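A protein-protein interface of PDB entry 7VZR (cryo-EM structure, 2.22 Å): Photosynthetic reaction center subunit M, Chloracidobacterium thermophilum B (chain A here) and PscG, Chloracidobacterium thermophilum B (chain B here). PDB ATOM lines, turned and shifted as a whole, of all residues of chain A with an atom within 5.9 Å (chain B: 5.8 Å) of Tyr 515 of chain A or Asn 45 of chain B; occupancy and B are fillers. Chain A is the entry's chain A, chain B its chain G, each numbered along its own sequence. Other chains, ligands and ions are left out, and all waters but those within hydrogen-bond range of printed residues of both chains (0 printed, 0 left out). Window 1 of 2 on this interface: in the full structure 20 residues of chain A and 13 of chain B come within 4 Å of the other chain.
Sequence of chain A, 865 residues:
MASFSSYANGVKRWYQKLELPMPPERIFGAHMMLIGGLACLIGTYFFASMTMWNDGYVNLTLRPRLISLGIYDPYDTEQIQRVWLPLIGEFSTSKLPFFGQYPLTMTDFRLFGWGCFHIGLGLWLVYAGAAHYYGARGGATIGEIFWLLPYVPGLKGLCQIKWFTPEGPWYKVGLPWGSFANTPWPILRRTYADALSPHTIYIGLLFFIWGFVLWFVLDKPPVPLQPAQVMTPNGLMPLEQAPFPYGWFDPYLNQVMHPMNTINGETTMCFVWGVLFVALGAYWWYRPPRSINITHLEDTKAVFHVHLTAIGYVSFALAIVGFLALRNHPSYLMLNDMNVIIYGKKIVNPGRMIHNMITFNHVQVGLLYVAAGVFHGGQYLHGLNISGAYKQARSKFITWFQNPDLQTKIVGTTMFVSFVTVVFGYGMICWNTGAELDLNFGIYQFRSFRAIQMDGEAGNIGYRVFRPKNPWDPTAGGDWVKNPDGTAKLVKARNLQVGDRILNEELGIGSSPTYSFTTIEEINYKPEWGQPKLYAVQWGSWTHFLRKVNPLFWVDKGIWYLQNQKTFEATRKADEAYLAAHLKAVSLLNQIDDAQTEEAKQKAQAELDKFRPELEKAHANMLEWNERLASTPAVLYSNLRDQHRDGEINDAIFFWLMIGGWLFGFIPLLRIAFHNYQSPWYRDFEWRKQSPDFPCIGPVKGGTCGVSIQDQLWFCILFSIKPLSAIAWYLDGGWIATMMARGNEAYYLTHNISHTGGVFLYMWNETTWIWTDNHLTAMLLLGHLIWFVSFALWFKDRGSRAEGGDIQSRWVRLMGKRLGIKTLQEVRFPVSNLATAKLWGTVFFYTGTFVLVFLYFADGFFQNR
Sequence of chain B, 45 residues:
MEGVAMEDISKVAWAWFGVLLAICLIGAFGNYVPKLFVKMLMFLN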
ATOM      1  N   ASP A 438      -6.431   2.950   1.896  1.00  0.00           N
ATOM      2  CA  ASP A 438      -5.683   3.920   1.059  1.00  0.00           C
ATOM      3  C   ASP A 438      -6.454   5.184   0.773  1.00  0.00           C
ATOM      4  O   ASP A 438      -6.413   5.673  -0.328  1.00  0.00           O
ATOM      5  CB  ASP A 438      -5.234   3.329  -0.262  1.00  0.00           C
ATOM      6  CG  ASP A 438      -4.080   2.404  -0.156  1.00  0.00           C
ATOM      7  OD1 ASP A 438      -3.019   2.827   0.176  1.00  0.00           O
ATOM      8  OD2 ASP A 438      -4.264   1.289  -0.487  1.00  0.00           O
ATOM      9  N   GLN A 445      -3.174  11.537   2.302  1.00  0.00           N
ATOM     10  CA  GLN A 445      -3.326  10.275   1.622  1.00  0.00           C
ATOM     11  C   GLN A 445      -2.960   9.180   2.591  1.00  0.00           C
ATOM     12  O   GLN A 445      -1.824   9.104   3.027  1.00  0.00           O
ATOM     13  CB  GLN A 445      -2.421  10.251   0.395  1.00  0.00           C
ATOM     14  CG  GLN A 445      -2.460   9.031  -0.536  1.00  0.00           C
ATOM     15  CD  GLN A 445      -3.871   8.658  -1.015  1.00  0.00           C
ATOM     16  OE1 GLN A 445      -4.600   7.900  -0.451  1.00  0.00           O
ATOM     17  NE2 GLN A 445      -4.181   9.162  -2.101  1.00  0.00           N
ATOM     18  N   PHE A 446      -3.916   8.360   2.977  1.00  0.00           N
ATOM     19  CA  PHE A 446      -3.594   7.135   3.689  1.00  0.00           C
ATOM     20  C   PHE A 446      -2.884   6.139   2.786  1.00  0.00           C
ATOM     21  O   PHE A 446      -3.164   6.055   1.601  1.00  0.00           O
ATOM     22  CB  PHE A 446      -4.848   6.513   4.234  1.00  0.00           C
ATOM     23  CG  PHE A 446      -5.348   7.122   5.486  1.00  0.00           C
ATOM     24  CD1 PHE A 446      -4.762   6.832   6.694  1.00  0.00           C
ATOM     25  CD2 PHE A 446      -6.354   8.057   5.453  1.00  0.00           C
ATOM     26  CE1 PHE A 446      -5.183   7.381   7.817  1.00  0.00           C
ATOM     27  CE2 PHE A 446      -6.817   8.591   6.573  1.00  0.00           C
ATOM     28  CZ  PHE A 446      -6.226   8.265   7.795  1.00  0.00           C
ATOM     29  N   ARG A 447      -1.897   5.428   3.327  1.00  0.00           N
ATOM     30  CA  ARG A 447      -1.147   4.446   2.565  1.00  0.00           C
ATOM     31  C   ARG A 447      -1.097   3.109   3.288  1.00  0.00           C
ATOM     32  O   ARG A 447      -0.789   3.040   4.448  1.00  0.00           O
ATOM     33  CB  ARG A 447       0.267   4.933   2.201  1.00  0.00           C
ATOM     34  CG  ARG A 447       0.242   5.790   0.971  1.00  0.00           C
ATOM     35  CD  ARG A 447       1.062   6.983   1.092  1.00  0.00           C
ATOM     36  NE  ARG A 447       2.414   6.612   0.878  1.00  0.00           N
ATOM     37  CZ  ARG A 447       3.401   6.624   1.744  1.00  0.00           C
ATOM     38  NH1 ARG A 447       3.266   7.034   2.974  1.00  0.00           N
ATOM     39  NH2 ARG A 447       4.543   6.153   1.359  1.00  0.00           N
ATOM     40  N   SER A 448      -1.208   2.057   2.525  1.00  0.00           N
ATOM     41  CA  SER A 448      -1.188   0.649   2.870  1.00  0.00           C
ATOM     42  C   SER A 448       0.212   0.095   3.180  1.00  0.00           C
ATOM     43  O   SER A 448       1.208   0.659   2.837  1.00  0.00           O
ATOM     44  CB  SER A 448      -1.780  -0.129   1.713  1.00  0.00           C
ATOM     45  OG  SER A 448      -3.070  -0.308   1.904  1.00  0.00           O
ATOM     46  N   ARG A 450       2.834  -2.674   2.058  1.00  0.00           N
ATOM     47  CA  ARG A 450       3.167  -3.572   0.962  1.00  0.00           C
ATOM     48  C   ARG A 450       4.595  -4.038   1.128  1.00  0.00           C
ATOM     49  O   ARG A 450       5.412  -3.314   1.653  1.00  0.00           O
ATOM     50  CB  ARG A 450       2.960  -2.985  -0.455  1.00  0.00           C
ATOM     51  CG  ARG A 450       2.596  -1.591  -0.627  1.00  0.00           C
ATOM     52  CD  ARG A 450       1.155  -1.269  -0.896  1.00  0.00           C
ATOM     53  NE  ARG A 450       1.073  -0.417  -2.061  1.00  0.00           N
ATOM     54  CZ  ARG A 450       0.030   0.206  -2.586  1.00  0.00           C
ATOM     55  NH1 ARG A 450      -1.152   0.198  -2.089  1.00  0.00           N
ATOM     56  NH2 ARG A 450       0.239   0.866  -3.661  1.00  0.00           N
ATOM     57  N   ARG A 501      10.479   4.709  -5.926  1.00  0.00           N
ATOM     58  CA  ARG A 501       9.102   4.527  -6.188  1.00  0.00           C
ATOM     59  C   ARG A 501       8.826   3.650  -7.271  1.00  0.00           C
ATOM     60  O   ARG A 501       9.360   3.747  -8.250  1.00  0.00           O
ATOM     61  CB  ARG A 501       8.362   5.820  -6.383  1.00  0.00           C
ATOM     62  CG  ARG A 501       8.885   6.940  -5.637  1.00  0.00           C
ATOM     63  CD  ARG A 501       8.121   7.483  -4.508  1.00  0.00           C
ATOM     64  NE  ARG A 501       9.203   8.105  -3.762  1.00  0.00           N
ATOM     65  CZ  ARG A 501       9.258   8.858  -2.616  1.00  0.00           C
ATOM     66  NH1 ARG A 501      10.446   9.265  -2.270  1.00  0.00           N
ATOM     67  NH2 ARG A 501       8.233   9.230  -1.862  1.00  0.00           N
ATOM     68  N   ASN A 504       2.316   1.531  -9.009  1.00  0.00           N
ATOM     69  CA  ASN A 504       1.374   0.573  -8.415  1.00  0.00           C
ATOM     70  C   ASN A 504       0.896  -0.456  -9.425  1.00  0.00           C
ATOM     71  O   ASN A 504       0.697  -1.602  -9.089  1.00  0.00           O
ATOM     72  CB  ASN A 504       0.099   1.214  -7.847  1.00  0.00           C
ATOM     73  CG  ASN A 504       0.289   2.006  -6.622  1.00  0.00           C
ATOM     74  OD1 ASN A 504       1.230   1.916  -5.960  1.00  0.00           O
ATOM     75  ND2 ASN A 504      -0.659   2.805  -6.322  1.00  0.00           N
ATOM     76  N   SER A 512      -5.773   0.945  -5.112  1.00  0.00           N
ATOM     77  CA  SER A 512      -5.316   2.227  -4.591  1.00  0.00           C
ATOM     78  C   SER A 512      -5.242   3.278  -5.677  1.00  0.00           C
ATOM     79  O   SER A 512      -4.240   3.952  -5.775  1.00  0.00           O
ATOM     80  CB  SER A 512      -3.997   2.132  -3.823  1.00  0.00           C
ATOM     81  OG  SER A 512      -2.861   2.312  -4.572  1.00  0.00           O
ATOM     82  N   PRO A 513      -6.378   3.630  -6.287  1.00  0.00           N
ATOM     83  CA  PRO A 513      -6.371   4.492  -7.467  1.00  0.00           C
ATOM     84  C   PRO A 513      -5.976   5.969  -7.253  1.00  0.00           C
ATOM     85  O   PRO A 513      -5.749   6.648  -8.212  1.00  0.00           O
ATOM     86  CB  PRO A 513      -7.812   4.370  -7.939  1.00  0.00           C
ATOM     87  CG  PRO A 513      -8.485   4.038  -6.881  1.00  0.00           C
ATOM     88  CD  PRO A 513      -7.744   3.174  -6.053  1.00  0.00           C
ATOM     89  N   THR A 514      -5.928   6.499  -6.049  1.00  0.00           N
ATOM     90  CA  THR A 514      -5.716   7.933  -5.896  1.00  0.00           C
ATOM     91  C   THR A 514      -4.242   8.334  -5.953  1.00  0.00           C
ATOM     92  O   THR A 514      -3.945   9.475  -6.152  1.00  0.00           O
ATOM     93  CB  THR A 514      -6.351   8.479  -4.596  1.00  0.00           C
ATOM     94  OG1 THR A 514      -5.681   7.986  -3.467  1.00  0.00           O
ATOM     95  CG2 THR A 514      -7.824   8.208  -4.473  1.00  0.00           C
ATOM     96  N   TYR A 515      -3.323   7.415  -5.888  1.00  0.00           N
ATOM     97  CA  TYR A 515      -1.923   7.690  -6.044  1.00  0.00           C
ATOM     98  C   TYR A 515      -1.365   6.615  -6.943  1.00  0.00           C
ATOM     99  O   TYR A 515      -2.005   5.619  -7.167  1.00  0.00           O
ATOM    100  CB  TYR A 515      -1.248   7.800  -4.667  1.00  0.00           C
ATOM    101  CG  TYR A 515      -1.124   6.559  -3.789  1.00  0.00           C
ATOM    102  CD1 TYR A 515      -2.109   6.169  -2.957  1.00  0.00           C
ATOM    103  CD2 TYR A 515       0.041   5.862  -3.758  1.00  0.00           C
ATOM    104  CE1 TYR A 515      -1.982   5.060  -2.159  1.00  0.00           C
ATOM    105  CE2 TYR A 515       0.201   4.768  -2.974  1.00  0.00           C
ATOM    106  CZ  TYR A 515      -0.791   4.383  -2.167  1.00  0.00           C
ATOM    107  OH  TYR A 515      -0.581   3.340  -1.395  1.00  0.00           O
ATOM    108  N   SER A 516      -0.149   6.770  -7.353  1.00  0.00           N
ATOM    109  CA  SER A 516       0.529   6.084  -8.439  1.00  0.00           C
ATOM    110  C   SER A 516       1.675   5.180  -8.027  1.00  0.00           C
ATOM    111  O   SER A 516       1.894   4.190  -8.650  1.00  0.00           O
ATOM    112  CB  SER A 516       1.049   7.120  -9.397  1.00  0.00           C
ATOM    113  OG  SER A 516      -0.006   7.553 -10.147  1.00  0.00           O
ATOM    114  N   PHE A 517       2.433   5.520  -7.028  1.00  0.00           N
ATOM    115  CA  PHE A 517       3.664   4.822  -6.670  1.00  0.00           C
ATOM    116  C   PHE A 517       3.567   4.137  -5.331  1.00  0.00           C
ATOM    117  O   PHE A 517       2.892   4.608  -4.453  1.00  0.00           O
ATOM    118  CB  PHE A 517       4.806   5.799  -6.634  1.00  0.00           C
ATOM    119  CG  PHE A 517       5.207   6.303  -7.950  1.00  0.00           C
ATOM    120  CD1 PHE A 517       6.103   5.637  -8.704  1.00  0.00           C
ATOM    121  CD2 PHE A 517       4.730   7.460  -8.426  1.00  0.00           C
ATOM    122  CE1 PHE A 517       6.476   6.092  -9.871  1.00  0.00           C
ATOM    123  CE2 PHE A 517       5.075   7.906  -9.618  1.00  0.00           C
ATOM    124  CZ  PHE A 517       5.939   7.214 -10.359  1.00  0.00           C
ATOM    125  N   THR A 518       4.309   3.060  -5.142  1.00  0.00           N
ATOM    126  CA  THR A 518       4.594   2.611  -3.792  1.00  0.00           C
ATOM    127  C   THR A 518       6.012   3.015  -3.474  1.00  0.00           C
ATOM    128  O   THR A 518       6.824   3.089  -4.364  1.00  0.00           O
ATOM    129  CB  THR A 518       4.320   1.110  -3.571  1.00  0.00           C
ATOM    130  OG1 THR A 518       5.506   0.331  -3.424  1.00  0.00           O
ATOM    131  CG2 THR A 518       3.493   0.600  -4.561  1.00  0.00           C
ATOM    132  N   THR A 519       6.273   3.393  -2.243  1.00  0.00           N
ATOM    133  CA  THR A 519       7.560   3.968  -1.860  1.00  0.00           C
ATOM    134  C   THR A 519       8.314   2.993  -1.000  1.00  0.00           C
ATOM    135  O   THR A 519       7.744   2.442  -0.091  1.00  0.00           O
ATOM    136  CB  THR A 519       7.375   5.242  -1.054  1.00  0.00           C
ATOM    137  OG1 THR A 519       6.460   6.061  -1.715  1.00  0.00           O
ATOM    138  CG2 THR A 519       8.651   5.950  -0.886  1.00  0.00           C
ATOM    139  N   GLN A 538       6.865  -0.669   2.032  1.00  0.00           N
ATOM    140  CA  GLN A 538       6.190   0.557   2.251  1.00  0.00           C
ATOM    141  C   GLN A 538       5.504   0.398   3.670  1.00  0.00           C
ATOM    142  O   GLN A 538       4.816  -0.475   3.881  1.00  0.00           O
ATOM    143  CB  GLN A 538       5.138   0.857   1.155  1.00  0.00           C
ATOM    144  CG  GLN A 538       4.188   2.011   1.404  1.00  0.00           C
ATOM    145  CD  GLN A 538       3.229   2.418   0.293  1.00  0.00           C
ATOM    146  OE1 GLN A 538       2.106   2.471   0.382  1.00  0.00           O
ATOM    147  NE2 GLN A 538       3.735   2.770  -0.640  1.00  0.00           N
ATOM    148  N   ASN B  31       0.044  16.451   0.493  1.00  0.00           N
ATOM    149  CA  ASN B  31      -0.692  15.572  -0.430  1.00  0.00           C
ATOM    150  C   ASN B  31      -0.648  16.074  -1.889  1.00  0.00           C
ATOM    151  O   ASN B  31      -0.213  15.424  -2.753  1.00  0.00           O
ATOM    152  CB  ASN B  31      -2.124  15.368   0.118  1.00  0.00           C
ATOM    153  CG  ASN B  31      -2.904  14.355  -0.571  1.00  0.00           C
ATOM    154  OD1 ASN B  31      -2.413  13.718  -1.348  1.00  0.00           O
ATOM    155  ND2 ASN B  31      -4.151  14.235  -0.273  1.00  0.00           N
ATOM    156  N   LYS B  35       2.831  16.009  -6.082  1.00  0.00           N
ATOM    157  CA  LYS B  35       2.127  15.400  -7.185  1.00  0.00           C
ATOM    158  C   LYS B  35       1.906  16.280  -8.340  1.00  0.00           C
ATOM    159  O   LYS B  35       1.945  15.859  -9.458  1.00  0.00           O
ATOM    160  CB  LYS B  35       0.713  15.007  -6.767  1.00  0.00           C
ATOM    161  CG  LYS B  35       0.642  13.675  -6.128  1.00  0.00           C
ATOM    162  CD  LYS B  35      -0.779  13.224  -6.119  1.00  0.00           C
ATOM    163  CE  LYS B  35      -1.222  13.090  -4.710  1.00  0.00           C
ATOM    164  NZ  LYS B  35      -2.125  11.959  -4.414  1.00  0.00           N
ATOM    165  N   PHE B  43       7.378  13.515   0.216  1.00  0.00           N
ATOM    166  CA  PHE B  43       5.986  13.257   0.484  1.00  0.00           C
ATOM    167  C   PHE B  43       5.207  12.792  -0.700  1.00  0.00           C
ATOM    168  O   PHE B  43       4.018  12.692  -0.722  1.00  0.00           O
ATOM    169  CB  PHE B  43       5.343  14.487   1.067  1.00  0.00           C
ATOM    170  CG  PHE B  43       5.833  14.818   2.403  1.00  0.00           C
ATOM    171  CD1 PHE B  43       5.790  13.900   3.402  1.00  0.00           C
ATOM    172  CD2 PHE B  43       6.366  16.051   2.667  1.00  0.00           C
ATOM    173  CE1 PHE B  43       6.229  14.218   4.640  1.00  0.00           C
ATOM    174  CE2 PHE B  43       6.849  16.360   3.907  1.00  0.00           C
ATOM    175  CZ  PHE B  43       6.766  15.448   4.904  1.00  0.00           C
ATOM    176  N   LEU B  44       5.918  12.432  -1.692  1.00  0.00           N
ATOM    177  CA  LEU B  44       5.319  11.946  -2.867  1.00  0.00           C
ATOM    178  C   LEU B  44       4.885  10.455  -2.759  1.00  0.00           C
ATOM    179  O   LEU B  44       5.549   9.654  -2.155  1.00  0.00           O
ATOM    180  CB  LEU B  44       6.378  12.179  -3.772  1.00  0.00           C
ATOM    181  CG  LEU B  44       6.126  13.143  -4.956  1.00  0.00           C
ATOM    182  CD1 LEU B  44       4.871  13.247  -5.822  1.00  0.00           C
ATOM    183  CD2 LEU B  44       7.052  14.339  -5.097  1.00  0.00           C
ATOM    184  N   ASN B  45       3.747  10.110  -3.354  1.00  0.00           N
ATOM    185  CA  ASN B  45       3.183   8.724  -3.297  1.00  0.00           C
ATOM    186  C   ASN B  45       2.544   8.351  -4.647  1.00  0.00           C
ATOM    187  O   ASN B  45       1.685   9.103  -5.132  1.00  0.00           O
ATOM    188  CB  ASN B  45       2.251   8.477  -2.106  1.00  0.00           C
ATOM    189  CG  ASN B  45       1.571   9.717  -1.559  1.00  0.00           C
ATOM    190  OD1 ASN B  45       0.948  10.467  -2.294  1.00  0.00           O
ATOM    191  ND2 ASN B  45       1.661   9.925  -0.255  1.00  0.00           N
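Printed residues of chain B within 4 Å of Gln 445 of chain A: Asn 31 (3.9 Å). Phe 446 of chain A touches none of the printed residues of chain B. Of the printed residues of chain B, Arg 447 of chain A touches Asn 45. Pro 513 of chain A touches none of the printed residues of chain B. Tyr 515 of chain A touches one residue of chain B. Of the printed residues of chain B, Phe 517 of chain A touches Asn 45. Printed residues of chain A within 4 Å of Lys 35 of chain B: Thr 514 (3.5 Å). The nearest residue of chain A that does not touch Asn 45 of chain B is Gln 445 of chain A (4.1 Å).
N of Asn 504 of chain A sits at hydrogen-bond distance from O of Ser 516 of chain A (2.7 Å). NE2 of Gln 538 of chain A lies close to N of Thr 519 of chain A (3.1 Å). ND2 of Asn 504 of chain A lies within hydrogen-bond range of O of Tyr 515 of chain A, at 3.2 Å. The guanidinium group of Arg 450 of chain A lies within hydrogen-bond range of the side-chain hydroxyl of Tyr 515 of chain A (3.3 Å). OD1 of Asp 438 of chain A lies within hydrogen-bond range of OH of Tyr 515 of chain A (2.9 Å). The side-chain hydroxyl (OH) of Tyr 515 of chain A is in hydrogen-bond range of the side-chain amide oxygen (OE1) of Gln 538 of chain A, 3.3 Å away.
Gln 445 of chain A touches Asn 31 of chain B (N to ND2, 3.9 Å). Asn 45 of chain B touches Arg 447 of chain A. Thr 514 of chain A touches Lys 35 of chain B (O to NZ, 3.5 Å). Tyr 515 of chain A touches Asn 45 of chain B (CB to O, 3.2 Å). N of Ser 516 of chain A touches O of Asn 45 of chain B, at 3.7 Å. N of Phe 517 of chain A touches C of Asn 45 of chain B (3.7 Å). Thr 519 of chain A touches Leu 44 of chain B (OG1 to O, 3.7 Å).
NH2 of Arg 501 of chain A lies within hydrogen-bond range of O of Leu 44 of chain B (2.7 Å).
Hydrophobic or aromatic side chains of chain A that line the printed part of chain B: Tyr 515 and Phe 517. Among the printed residues, no Asp or Glu carboxylate lies within 4 Å of a Lys or Arg side-chain nitrogen of the other chain.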
